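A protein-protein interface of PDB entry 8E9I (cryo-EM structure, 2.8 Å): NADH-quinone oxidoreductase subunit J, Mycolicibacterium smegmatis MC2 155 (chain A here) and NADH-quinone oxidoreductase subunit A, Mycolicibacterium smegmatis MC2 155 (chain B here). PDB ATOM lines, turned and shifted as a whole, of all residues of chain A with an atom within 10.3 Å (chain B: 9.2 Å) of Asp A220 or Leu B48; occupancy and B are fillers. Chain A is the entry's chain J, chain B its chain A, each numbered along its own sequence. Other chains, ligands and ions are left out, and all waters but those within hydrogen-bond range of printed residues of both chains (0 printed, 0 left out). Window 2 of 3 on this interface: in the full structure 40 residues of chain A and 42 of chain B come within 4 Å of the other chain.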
ATOM      1  N   PRO A 208     -32.726  -7.833 -26.783  1.00  0.00           N
ATOM      2  CA  PRO A 208     -31.970  -8.391 -27.904  1.00  0.00           C
ATOM      3  C   PRO A 208     -32.019  -9.911 -27.892  1.00  0.00           C
ATOM      4  O   PRO A 208     -32.018 -10.556 -26.843  1.00  0.00           O
ATOM      5  CB  PRO A 208     -30.546  -7.872 -27.674  1.00  0.00           C
ATOM      6  CG  PRO A 208     -30.506  -7.468 -26.249  1.00  0.00           C
ATOM      7  CD  PRO A 208     -31.879  -7.006 -25.914  1.00  0.00           C
ATOM      8  N   ASN A 209     -32.086 -10.473 -29.075  1.00  0.00           N
ATOM      9  CA  ASN A 209     -32.209 -11.908 -29.243  1.00  0.00           C
ATOM     10  C   ASN A 209     -30.922 -12.613 -28.852  1.00  0.00           C
ATOM     11  O   ASN A 209     -29.841 -12.023 -28.896  1.00  0.00           O
ATOM     12  CB  ASN A 209     -32.541 -12.237 -30.691  1.00  0.00           C
ATOM     13  CG  ASN A 209     -31.472 -11.760 -31.652  1.00  0.00           C
ATOM     14  OD1 ASN A 209     -30.942 -10.659 -31.514  1.00  0.00           O
ATOM     15  ND2 ASN A 209     -31.124 -12.605 -32.608  1.00  0.00           N
ATOM     16  N   PRO A 210     -31.000 -13.882 -28.471  1.00  0.00           N
ATOM     17  CA  PRO A 210     -29.778 -14.665 -28.293  1.00  0.00           C
ATOM     18  C   PRO A 210     -29.025 -14.780 -29.603  1.00  0.00           C
ATOM     19  O   PRO A 210     -29.609 -14.833 -30.685  1.00  0.00           O
ATOM     20  CB  PRO A 210     -30.288 -16.026 -27.818  1.00  0.00           C
ATOM     21  CG  PRO A 210     -31.688 -16.087 -28.273  1.00  0.00           C
ATOM     22  CD  PRO A 210     -32.202 -14.690 -28.217  1.00  0.00           C
ATOM     23  N   GLY A 211     -27.704 -14.828 -29.490  1.00  0.00           N
ATOM     24  CA  GLY A 211     -26.870 -14.822 -30.667  1.00  0.00           C
ATOM     25  C   GLY A 211     -27.048 -16.073 -31.503  1.00  0.00           C
ATOM     26  O   GLY A 211     -27.424 -17.136 -31.013  1.00  0.00           O
ATOM     27  N   VAL A 212     -26.778 -15.930 -32.797  1.00  0.00           N
ATOM     28  CA  VAL A 212     -26.795 -17.039 -33.742  1.00  0.00           C
ATOM     29  C   VAL A 212     -25.379 -17.226 -34.253  1.00  0.00           C
ATOM     30  O   VAL A 212     -24.792 -16.300 -34.824  1.00  0.00           O
ATOM     31  CB  VAL A 212     -27.765 -16.791 -34.903  1.00  0.00           C
ATOM     32  CG1 VAL A 212     -27.714 -17.944 -35.884  1.00  0.00           C
ATOM     33  CG2 VAL A 212     -29.168 -16.595 -34.375  1.00  0.00           C
ATOM     34  N   TYR A 213     -24.832 -18.414 -34.040  1.00  0.00           N
ATOM     35  CA  TYR A 213     -23.499 -18.761 -34.491  1.00  0.00           C
ATOM     36  C   TYR A 213     -23.589 -20.010 -35.344  1.00  0.00           C
ATOM     37  O   TYR A 213     -24.548 -20.777 -35.242  1.00  0.00           O
ATOM     38  CB  TYR A 213     -22.555 -19.025 -33.322  1.00  0.00           C
ATOM     39  CG  TYR A 213     -22.330 -17.847 -32.420  1.00  0.00           C
ATOM     40  CD1 TYR A 213     -23.337 -17.376 -31.600  1.00  0.00           C
ATOM     41  CD2 TYR A 213     -21.101 -17.217 -32.373  1.00  0.00           C
ATOM     42  CE1 TYR A 213     -23.135 -16.305 -30.774  1.00  0.00           C
ATOM     43  CE2 TYR A 213     -20.888 -16.142 -31.549  1.00  0.00           C
ATOM     44  CZ  TYR A 213     -21.908 -15.691 -30.748  1.00  0.00           C
ATOM     45  OH  TYR A 213     -21.703 -14.616 -29.916  1.00  0.00           O
ATOM     46  N   HIS A 216     -24.098 -23.187 -33.241  1.00  0.00           N
ATOM     47  CA  HIS A 216     -24.801 -22.858 -32.005  1.00  0.00           C
ATOM     48  C   HIS A 216     -25.817 -21.764 -32.276  1.00  0.00           C
ATOM     49  O   HIS A 216     -25.439 -20.620 -32.539  1.00  0.00           O
ATOM     50  CB  HIS A 216     -23.829 -22.404 -30.916  1.00  0.00           C
ATOM     51  CG  HIS A 216     -22.762 -23.401 -30.606  1.00  0.00           C
ATOM     52  ND1 HIS A 216     -23.018 -24.581 -29.945  1.00  0.00           N
ATOM     53  CD2 HIS A 216     -21.433 -23.392 -30.864  1.00  0.00           C
ATOM     54  CE1 HIS A 216     -21.893 -25.261 -29.812  1.00  0.00           C
ATOM     55  NE2 HIS A 216     -20.916 -24.560 -30.360  1.00  0.00           N
ATOM     56  N   ASN A 217     -27.100 -22.108 -32.195  1.00  0.00           N
ATOM     57  CA  ASN A 217     -28.156 -21.116 -32.333  1.00  0.00           C
ATOM     58  C   ASN A 217     -29.167 -21.187 -31.196  1.00  0.00           C
ATOM     59  O   ASN A 217     -30.138 -20.422 -31.206  1.00  0.00           O
ATOM     60  CB  ASN A 217     -28.873 -21.286 -33.672  1.00  0.00           C
ATOM     61  CG  ASN A 217     -29.462 -22.664 -33.841  1.00  0.00           C
ATOM     62  OD1 ASN A 217     -29.796 -23.331 -32.866  1.00  0.00           O
ATOM     63  ND2 ASN A 217     -29.596 -23.099 -35.084  1.00  0.00           N
ATOM     64  N   SER A 218     -28.969 -22.070 -30.224  1.00  0.00           N
ATOM     65  CA  SER A 218     -29.925 -22.237 -29.144  1.00  0.00           C
ATOM     66  C   SER A 218     -30.115 -20.930 -28.381  1.00  0.00           C
ATOM     67  O   SER A 218     -29.312 -20.000 -28.470  1.00  0.00           O
ATOM     68  CB  SER A 218     -29.458 -23.336 -28.191  1.00  0.00           C
ATOM     69  OG  SER A 218     -28.103 -23.156 -27.830  1.00  0.00           O
ATOM     70  N   VAL A 219     -31.204 -20.872 -27.615  1.00  0.00           N
ATOM     71  CA  VAL A 219     -31.523 -19.680 -26.839  1.00  0.00           C
ATOM     72  C   VAL A 219     -30.471 -19.352 -25.795  1.00  0.00           C
ATOM     73  O   VAL A 219     -30.348 -18.189 -25.400  1.00  0.00           O
ATOM     74  CB  VAL A 219     -32.889 -19.846 -26.148  1.00  0.00           C
ATOM     75  CG1 VAL A 219     -33.981 -20.041 -27.177  1.00  0.00           C
ATOM     76  CG2 VAL A 219     -32.857 -21.016 -25.188  1.00  0.00           C
ATOM     77  N   ASP A 220     -29.709 -20.340 -25.335  1.00  0.00           N
ATOM     78  CA  ASP A 220     -28.707 -20.114 -24.305  1.00  0.00           C
ATOM     79  C   ASP A 220     -27.476 -19.380 -24.815  1.00  0.00           C
ATOM     80  O   ASP A 220     -26.619 -19.015 -24.005  1.00  0.00           O
ATOM     81  CB  ASP A 220     -28.279 -21.452 -23.700  1.00  0.00           C
ATOM     82  N   VAL A 221     -27.370 -19.157 -26.121  1.00  0.00           N
ATOM     83  CA  VAL A 221     -26.176 -18.584 -26.734  1.00  0.00           C
ATOM     84  C   VAL A 221     -26.207 -17.064 -26.607  1.00  0.00           C
ATOM     85  O   VAL A 221     -27.118 -16.425 -27.147  1.00  0.00           O
ATOM     86  CB  VAL A 221     -26.077 -19.006 -28.206  1.00  0.00           C
ATOM     87  CG1 VAL A 221     -24.824 -18.441 -28.837  1.00  0.00           C
ATOM     88  CG2 VAL A 221     -26.120 -20.519 -28.328  1.00  0.00           C
ATOM     89  N   PRO A 222     -25.246 -16.438 -25.928  1.00  0.00           N
ATOM     90  CA  PRO A 222     -25.262 -14.975 -25.827  1.00  0.00           C
ATOM     91  C   PRO A 222     -24.759 -14.319 -27.102  1.00  0.00           C
ATOM     92  O   PRO A 222     -23.893 -14.852 -27.799  1.00  0.00           O
ATOM     93  CB  PRO A 222     -24.329 -14.695 -24.648  1.00  0.00           C
ATOM     94  CG  PRO A 222     -23.372 -15.813 -24.676  1.00  0.00           C
ATOM     95  CD  PRO A 222     -24.138 -17.019 -25.151  1.00  0.00           C
ATOM     96  N   ALA A 223     -25.302 -13.143 -27.396  1.00  0.00           N
ATOM     97  CA  ALA A 223     -24.945 -12.419 -28.606  1.00  0.00           C
ATOM     98  C   ALA A 223     -23.626 -11.681 -28.424  1.00  0.00           C
ATOM     99  O   ALA A 223     -23.177 -11.438 -27.302  1.00  0.00           O
ATOM    100  CB  ALA A 223     -26.048 -11.433 -28.981  1.00  0.00           C
ATOM    101  N   ARG A 224     -23.005 -11.321 -29.544  1.00  0.00           N
ATOM    102  CA  ARG A 224     -21.684 -10.709 -29.537  1.00  0.00           C
ATOM    103  C   ARG A 224     -21.785  -9.212 -29.799  1.00  0.00           C
ATOM    104  O   ARG A 224     -22.336  -8.790 -30.820  1.00  0.00           O
ATOM    105  CB  ARG A 224     -20.790 -11.362 -30.589  1.00  0.00           C
ATOM    106  CG  ARG A 224     -19.385 -10.797 -30.638  1.00  0.00           C
ATOM    107  CD  ARG A 224     -18.557 -11.482 -31.705  1.00  0.00           C
ATOM    108  NE  ARG A 224     -18.265 -12.866 -31.356  1.00  0.00           N
ATOM    109  CZ  ARG A 224     -17.963 -13.814 -32.232  1.00  0.00           C
ATOM    110  NH1 ARG A 224     -17.884 -13.560 -33.527  1.00  0.00           N
ATOM    111  NH2 ARG A 224     -17.733 -15.049 -31.796  1.00  0.00           N
ATOM    112  N   GLU A 230     -19.613 -10.666 -24.920  1.00  0.00           N
ATOM    113  CA  GLU A 230     -20.927 -11.291 -24.943  1.00  0.00           C
ATOM    114  C   GLU A 230     -21.924 -10.365 -24.263  1.00  0.00           C
ATOM    115  O   GLU A 230     -21.717  -9.959 -23.117  1.00  0.00           O
ATOM    116  CB  GLU A 230     -20.894 -12.652 -24.249  1.00  0.00           C
ATOM    117  N   SER A 231     -22.995 -10.035 -24.963  1.00  0.00           N
ATOM    118  CA  SER A 231     -24.000  -9.144 -24.404  1.00  0.00           C
ATOM    119  C   SER A 231     -24.783  -9.870 -23.319  1.00  0.00           C
ATOM    120  O   SER A 231     -25.422 -10.888 -23.611  1.00  0.00           O
ATOM    121  CB  SER A 231     -24.941  -8.656 -25.495  1.00  0.00           C
ATOM    122  OG  SER A 231     -25.452  -9.745 -26.235  1.00  0.00           O
ATOM    123  N   PRO A 232     -24.765  -9.402 -22.070  1.00  0.00           N
ATOM    124  CA  PRO A 232     -25.590 -10.051 -21.041  1.00  0.00           C
ATOM    125  C   PRO A 232     -27.074 -10.011 -21.343  1.00  0.00           C
ATOM    126  O   PRO A 232     -27.786 -10.962 -21.003  1.00  0.00           O
ATOM    127  CB  PRO A 232     -25.259  -9.253 -19.773  1.00  0.00           C
ATOM    128  CG  PRO A 232     -23.933  -8.633 -20.050  1.00  0.00           C
ATOM    129  CD  PRO A 232     -23.943  -8.321 -21.504  1.00  0.00           C
ATOM    130  N   LEU A 233     -27.561  -8.945 -21.974  1.00  0.00           N
ATOM    131  CA  LEU A 233     -28.989  -8.802 -22.211  1.00  0.00           C
ATOM    132  C   LEU A 233     -29.516  -9.794 -23.237  1.00  0.00           C
ATOM    133  O   LEU A 233     -30.682 -10.191 -23.151  1.00  0.00           O
ATOM    134  CB  LEU A 233     -29.288  -7.377 -22.668  1.00  0.00           C
ATOM    135  CG  LEU A 233     -28.858  -6.296 -21.678  1.00  0.00           C
ATOM    136  CD1 LEU A 233     -29.149  -4.920 -22.242  1.00  0.00           C
ATOM    137  CD2 LEU A 233     -29.555  -6.489 -20.345  1.00  0.00           C
ATOM    138  N   SER A 234     -28.692 -10.203 -24.202  1.00  0.00           N
ATOM    139  CA  SER A 234     -29.164 -11.098 -25.251  1.00  0.00           C
ATOM    140  C   SER A 234     -29.635 -12.424 -24.674  1.00  0.00           C
ATOM    141  O   SER A 234     -30.662 -12.963 -25.095  1.00  0.00           O
ATOM    142  CB  SER A 234     -28.057 -11.329 -26.275  1.00  0.00           C
ATOM    143  OG  SER A 234     -26.913 -11.888 -25.659  1.00  0.00           O
ATOM    144  N   VAL A 235     -28.889 -12.968 -23.715  1.00  0.00           N
ATOM    145  CA  VAL A 235     -29.298 -14.203 -23.063  1.00  0.00           C
ATOM    146  C   VAL A 235     -30.189 -13.875 -21.876  1.00  0.00           C
ATOM    147  O   VAL A 235     -29.900 -12.965 -21.089  1.00  0.00           O
ATOM    148  CB  VAL A 235     -28.070 -15.021 -22.632  1.00  0.00           C
ATOM    149  CG1 VAL A 235     -27.166 -14.204 -21.716  1.00  0.00           C
ATOM    150  CG2 VAL A 235     -28.510 -16.301 -21.946  1.00  0.00           C
ATOM    151  N   SER A 236     -31.283 -14.618 -21.745  1.00  0.00           N
ATOM    152  CA  SER A 236     -32.236 -14.361 -20.675  1.00  0.00           C
ATOM    153  C   SER A 236     -31.541 -14.361 -19.320  1.00  0.00           C
ATOM    154  O   SER A 236     -30.431 -14.878 -19.168  1.00  0.00           O
ATOM    155  CB  SER A 236     -33.344 -15.411 -20.691  1.00  0.00           C
ATOM    156  OG  SER A 236     -34.281 -15.166 -19.660  1.00  0.00           O
ATOM    157  N   THR A 237     -32.200 -13.760 -18.331  1.00  0.00           N
ATOM    158  CA  THR A 237     -31.630 -13.713 -16.991  1.00  0.00           C
ATOM    159  C   THR A 237     -31.513 -15.104 -16.383  1.00  0.00           C
ATOM    160  O   THR A 237     -30.546 -15.391 -15.669  1.00  0.00           O
ATOM    161  CB  THR A 237     -32.479 -12.816 -16.092  1.00  0.00           C
ATOM    162  N   ILE A 238     -32.478 -15.984 -16.658  1.00  0.00           N
ATOM    163  CA  ILE A 238     -32.537 -17.279 -15.987  1.00  0.00           C
ATOM    164  C   ILE A 238     -31.546 -18.291 -16.533  1.00  0.00           C
ATOM    165  O   ILE A 238     -31.286 -19.302 -15.870  1.00  0.00           O
ATOM    166  CB  ILE A 238     -33.953 -17.874 -16.095  1.00  0.00           C
ATOM    167  CG1 ILE A 238     -34.330 -18.107 -17.562  1.00  0.00           C
ATOM    168  CG2 ILE A 238     -34.953 -16.948 -15.439  1.00  0.00           C
ATOM    169  CD1 ILE A 238     -35.598 -18.901 -17.745  1.00  0.00           C
ATOM    170  N   LEU A 239     -30.997 -18.060 -17.694  1.00  0.00           N
ATOM    171  CA  LEU A 239     -30.136 -19.097 -18.239  1.00  0.00           C
ATOM    172  C   LEU A 239     -28.735 -19.017 -17.641  1.00  0.00           C
ATOM    173  O   LEU A 239     -28.271 -17.937 -17.266  1.00  0.00           O
ATOM    174  CB  LEU A 239     -30.058 -18.979 -19.756  1.00  0.00           C
ATOM    175  CG  LEU A 239     -31.379 -19.352 -20.430  1.00  0.00           C
ATOM    176  CD1 LEU A 239     -31.464 -18.794 -21.841  1.00  0.00           C
ATOM    177  CD2 LEU A 239     -31.539 -20.864 -20.437  1.00  0.00           C
ATOM    178  N   PRO A 240     -28.050 -20.158 -17.540  1.00  0.00           N
ATOM    179  CA  PRO A 240     -26.744 -20.182 -16.872  1.00  0.00           C
ATOM    180  C   PRO A 240     -25.590 -19.837 -17.796  1.00  0.00           C
ATOM    181  O   PRO A 240     -24.573 -20.534 -17.806  1.00  0.00           O
ATOM    182  CB  PRO A 240     -26.651 -21.632 -16.390  1.00  0.00           C
ATOM    183  CG  PRO A 240     -27.314 -22.381 -17.497  1.00  0.00           C
ATOM    184  CD  PRO A 240     -28.477 -21.514 -17.928  1.00  0.00           C
ATOM    185  N   HIS A 241     -25.726 -18.769 -18.566  1.00  0.00           N
ATOM    186  CA  HIS A 241     -24.682 -18.385 -19.517  1.00  0.00           C
ATOM    187  C   HIS A 241     -24.496 -19.538 -20.507  1.00  0.00           C
ATOM    188  O   HIS A 241     -25.430 -20.302 -20.770  1.00  0.00           O
ATOM    189  CB  HIS A 241     -23.433 -17.994 -18.749  1.00  0.00           C
ATOM    190  N   ARG A 242     -23.300 -19.681 -21.071  1.00  0.00           N
ATOM    191  CA  ARG A 242     -23.041 -20.742 -22.042  1.00  0.00           C
ATOM    192  C   ARG A 242     -21.549 -20.986 -22.222  1.00  0.00           C
ATOM    193  O   ARG A 242     -20.819 -20.112 -22.686  1.00  0.00           O
ATOM    194  CB  ARG A 242     -23.675 -20.397 -23.389  1.00  0.00           C
ATOM    195  N   GLU B  39     -33.211 -35.487 -31.579  1.00  0.00           N
ATOM    196  CA  GLU B  39     -33.244 -34.373 -30.651  1.00  0.00           C
ATOM    197  C   GLU B  39     -34.660 -33.813 -30.550  1.00  0.00           C
ATOM    198  O   GLU B  39     -35.496 -33.989 -31.438  1.00  0.00           O
ATOM    199  CB  GLU B  39     -32.265 -33.284 -31.085  1.00  0.00           C
ATOM    200  N   ALA B  40     -34.925 -33.124 -29.446  1.00  0.00           N
ATOM    201  CA  ALA B  40     -36.243 -32.549 -29.235  1.00  0.00           C
ATOM    202  C   ALA B  40     -36.574 -31.577 -30.355  1.00  0.00           C
ATOM    203  O   ALA B  40     -35.694 -30.933 -30.928  1.00  0.00           O
ATOM    204  CB  ALA B  40     -36.300 -31.829 -27.888  1.00  0.00           C
ATOM    205  N   TYR B  41     -37.856 -31.489 -30.685  1.00  0.00           N
ATOM    206  CA  TYR B  41     -38.291 -30.487 -31.644  1.00  0.00           C
ATOM    207  C   TYR B  41     -38.366 -29.132 -30.959  1.00  0.00           C
ATOM    208  O   TYR B  41     -39.015 -28.986 -29.920  1.00  0.00           O
ATOM    209  CB  TYR B  41     -39.648 -30.847 -32.232  1.00  0.00           C
ATOM    210  CG  TYR B  41     -40.243 -29.738 -33.056  1.00  0.00           C
ATOM    211  CD1 TYR B  41     -39.731 -29.428 -34.302  1.00  0.00           C
ATOM    212  CD2 TYR B  41     -41.314 -29.000 -32.588  1.00  0.00           C
ATOM    213  CE1 TYR B  41     -40.262 -28.415 -35.055  1.00  0.00           C
ATOM    214  CE2 TYR B  41     -41.854 -27.988 -33.335  1.00  0.00           C
ATOM    215  CZ  TYR B  41     -41.327 -27.703 -34.571  1.00  0.00           C
ATOM    216  OH  TYR B  41     -41.860 -26.691 -35.326  1.00  0.00           O
ATOM    217  N   GLU B  42     -37.697 -28.142 -31.536  1.00  0.00           N
ATOM    218  CA  GLU B  42     -37.739 -26.779 -31.025  1.00  0.00           C
ATOM    219  C   GLU B  42     -37.881 -25.807 -32.188  1.00  0.00           C
ATOM    220  O   GLU B  42     -37.219 -24.773 -32.254  1.00  0.00           O
ATOM    221  CB  GLU B  42     -36.498 -26.471 -30.195  1.00  0.00           C
ATOM    222  CG  GLU B  42     -36.575 -25.185 -29.394  1.00  0.00           C
ATOM    223  CD  GLU B  42     -37.773 -25.139 -28.468  1.00  0.00           C
ATOM    224  OE1 GLU B  42     -38.191 -26.210 -27.987  1.00  0.00           O
ATOM    225  OE2 GLU B  42     -38.289 -24.036 -28.216  1.00  0.00           O
ATOM    226  N   ILE B  45     -34.567 -24.822 -33.953  1.00  0.00           N
ATOM    227  CA  ILE B  45     -33.447 -24.304 -33.185  1.00  0.00           C
ATOM    228  C   ILE B  45     -32.823 -25.425 -32.371  1.00  0.00           C
ATOM    229  O   ILE B  45     -33.497 -26.385 -31.977  1.00  0.00           O
ATOM    230  CB  ILE B  45     -33.916 -23.152 -32.282  1.00  0.00           C
ATOM    231  CG1 ILE B  45     -34.461 -22.000 -33.125  1.00  0.00           C
ATOM    232  CG2 ILE B  45     -32.785 -22.669 -31.405  1.00  0.00           C
ATOM    233  CD1 ILE B  45     -33.547 -21.551 -34.238  1.00  0.00           C
ATOM    234  N   ASP B  46     -31.530 -25.308 -32.111  1.00  0.00           N
ATOM    235  CA  ASP B  46     -30.853 -26.311 -31.309  1.00  0.00           C
ATOM    236  C   ASP B  46     -31.491 -26.376 -29.923  1.00  0.00           C
ATOM    237  O   ASP B  46     -31.622 -25.344 -29.255  1.00  0.00           O
ATOM    238  CB  ASP B  46     -29.364 -25.980 -31.187  1.00  0.00           C
ATOM    239  N   PRO B  47     -31.911 -27.553 -29.461  1.00  0.00           N
ATOM    240  CA  PRO B  47     -32.450 -27.646 -28.103  1.00  0.00           C
ATOM    241  C   PRO B  47     -31.362 -27.393 -27.073  1.00  0.00           C
ATOM    242  O   PRO B  47     -30.177 -27.618 -27.321  1.00  0.00           O
ATOM    243  CB  PRO B  47     -32.978 -29.080 -28.028  1.00  0.00           C
ATOM    244  CG  PRO B  47     -32.173 -29.819 -29.016  1.00  0.00           C
ATOM    245  CD  PRO B  47     -31.909 -28.862 -30.134  1.00  0.00           C
ATOM    246  N   LEU B  48     -31.781 -26.929 -25.906  1.00  0.00           N
ATOM    247  CA  LEU B  48     -30.862 -26.512 -24.858  1.00  0.00           C
ATOM    248  C   LEU B  48     -29.824 -27.580 -24.544  1.00  0.00           C
ATOM    249  O   LEU B  48     -29.990 -28.744 -24.928  1.00  0.00           O
ATOM    250  CB  LEU B  48     -31.642 -26.176 -23.593  1.00  0.00           C
ATOM    251  CG  LEU B  48     -32.366 -24.839 -23.605  1.00  0.00           C
ATOM    252  CD1 LEU B  48     -33.305 -24.754 -22.421  1.00  0.00           C
ATOM    253  CD2 LEU B  48     -31.351 -23.712 -23.567  1.00  0.00           C
ATOM    254  N   PRO B  49     -28.745 -27.222 -23.856  1.00  0.00           N
ATOM    255  CA  PRO B  49     -27.740 -28.213 -23.475  1.00  0.00           C
ATOM    256  C   PRO B  49     -28.367 -29.354 -22.700  1.00  0.00           C
ATOM    257  O   PRO B  49     -29.476 -29.212 -22.163  1.00  0.00           O
ATOM    258  CB  PRO B  49     -26.773 -27.409 -22.597  1.00  0.00           C
ATOM    259  CG  PRO B  49     -26.898 -26.025 -23.090  1.00  0.00           C
ATOM    260  CD  PRO B  49     -28.328 -25.856 -23.504  1.00  0.00           C
ATOM    261  N   PRO B  50     -27.686 -30.500 -22.608  1.00  0.00           N
ATOM    262  CA  PRO B  50     -28.287 -31.656 -21.931  1.00  0.00           C
ATOM    263  C   PRO B  50     -28.729 -31.308 -20.523  1.00  0.00           C
ATOM    264  O   PRO B  50     -29.793 -31.738 -20.068  1.00  0.00           O
ATOM    265  CB  PRO B  50     -27.159 -32.695 -21.937  1.00  0.00           C
ATOM    266  CG  PRO B  50     -25.906 -31.899 -22.082  1.00  0.00           C
ATOM    267  CD  PRO B  50     -26.273 -30.731 -22.946  1.00  0.00           C
ATOM    268  N   VAL B  51     -27.915 -30.517 -19.829  1.00  0.00           N
ATOM    269  CA  VAL B  51     -28.342 -29.900 -18.581  1.00  0.00           C
ATOM    270  C   VAL B  51     -29.133 -28.661 -18.965  1.00  0.00           C
ATOM    271  O   VAL B  51     -28.569 -27.569 -19.090  1.00  0.00           O
ATOM    272  CB  VAL B  51     -27.147 -29.551 -17.677  1.00  0.00           C
ATOM    273  N   ALA B  52     -30.445 -28.834 -19.155  1.00  0.00           N
ATOM    274  CA  ALA B  52     -31.304 -27.823 -19.762  1.00  0.00           C
ATOM    275  C   ALA B  52     -30.884 -26.426 -19.342  1.00  0.00           C
ATOM    276  O   ALA B  52     -30.679 -25.546 -20.185  1.00  0.00           O
ATOM    277  CB  ALA B  52     -32.764 -28.068 -19.379  1.00  0.00           C
ATOM    278  N   ALA B  53     -30.744 -26.223 -18.039  1.00  0.00           N
ATOM    279  CA  ALA B  53     -30.222 -24.974 -17.510  1.00  0.00           C
ATOM    280  C   ALA B  53     -30.154 -25.064 -15.994  1.00  0.00           C
ATOM    281  O   ALA B  53     -30.729 -25.981 -15.398  1.00  0.00           O
ATOM    282  CB  ALA B  53     -31.094 -23.797 -17.951  1.00  0.00           C
ATOM    283  N   GLY B  54     -29.443 -24.136 -15.362  1.00  0.00           N
ATOM    284  CA  GLY B  54     -29.559 -23.990 -13.928  1.00  0.00           C
ATOM    285  C   GLY B  54     -31.012 -23.742 -13.585  1.00  0.00           C
ATOM    286  O   GLY B  54     -31.584 -22.728 -13.998  1.00  0.00           O
ATOM    287  N   LEU B  55     -31.624 -24.664 -12.845  1.00  0.00           N
ATOM    288  CA  LEU B  55     -33.062 -24.620 -12.622  1.00  0.00           C
ATOM    289  C   LEU B  55     -33.775 -24.942 -13.930  1.00  0.00           C
ATOM    290  O   LEU B  55     -33.801 -26.104 -14.350  1.00  0.00           O
ATOM    291  CB  LEU B  55     -33.488 -23.256 -12.070  1.00  0.00           C
ATOM    292  N   THR B  56     -34.351 -23.932 -14.582  1.00  0.00           N
ATOM    293  CA  THR B  56     -35.008 -24.123 -15.871  1.00  0.00           C
ATOM    294  C   THR B  56     -36.352 -24.820 -15.710  1.00  0.00           C
ATOM    295  O   THR B  56     -36.925 -24.833 -14.619  1.00  0.00           O
ATOM    296  CB  THR B  56     -34.116 -24.929 -16.817  1.00  0.00           C
ATOM    297  N   GLY B  57     -36.854 -25.424 -16.783  1.00  0.00           N
ATOM    298  CA  GLY B  57     -38.209 -25.936 -16.785  1.00  0.00           C
ATOM    299  C   GLY B  57     -38.397 -27.193 -15.965  1.00  0.00           C
ATOM    300  O   GLY B  57     -38.951 -28.184 -16.450  1.00  0.00           O
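N of Asp B46 is in hydrogen-bond range of OD1 of Asn A217 (2.7 Å).
Among the printed residues, pairs that only touch across the chains: Asn A217 with Ile B45 (3.4 Å), Ser A218 with Ile B45 (3.7 Å), Ser A218 with Asp B46 (3.1 Å), Val A219 with Leu B48 (3.5 Å), Asp A220 with Leu B48 (3.8 Å), Ile A238 with Gly B54 (3.9 Å), Leu A239 with Ala B53 (3.9 Å), Pro A240 with Ala B53 (3.5 Å) and Pro A240 with Gly B54 (3.5 Å).
Asp A220 touches one residue of chain B.
No residue of chain B comes within 4 Å of Val A221.
Thr A237 touches none of the printed residues of chain B.
Of the printed residues of chain B, Leu A239 touches Ala B53 (3.9 Å).
No residue of chain A comes within 4 Å of Pro B47.
Of the printed residues of chain A, Leu B48 touches Val A219 and Asp A220.
Pro B49 touches none of the printed residues of chain A.
No residue of chain A comes within 4 Å of Pro B50.
No residue of chain A comes within 4 Å of Ala B52.
Printed residues of chain A within 4 Å of Ala B53: Leu A239 (3.9 Å) and Pro A240 (3.5 Å).
Leu B55 touches none of the printed residues of chain A.
The nearest residue of chain B that does not touch Asp A220 is Pro B49 (4.4 Å).
The nearest residue of chain A that does not touch Leu B48 is Leu A239 (4.2 Å).
The nearest printed residue of chain B that does not touch Ile A238 is Ala B53 (5.0 Å).
Of the 17 printed residues of chain B, 5 touch a printed residue of chain A.
Printed residues of chain B that touch a printed residue of chain A: Ile B45, Asp B46, Leu B48, Ala B53 and Gly B54.
Among the printed residues, 10 pairs touch across the chains.
Among the printed residues, no Asp or Glu carboxylate lies within 4 Å of a Lys or Arg side-chain nitrogen of the other chain.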
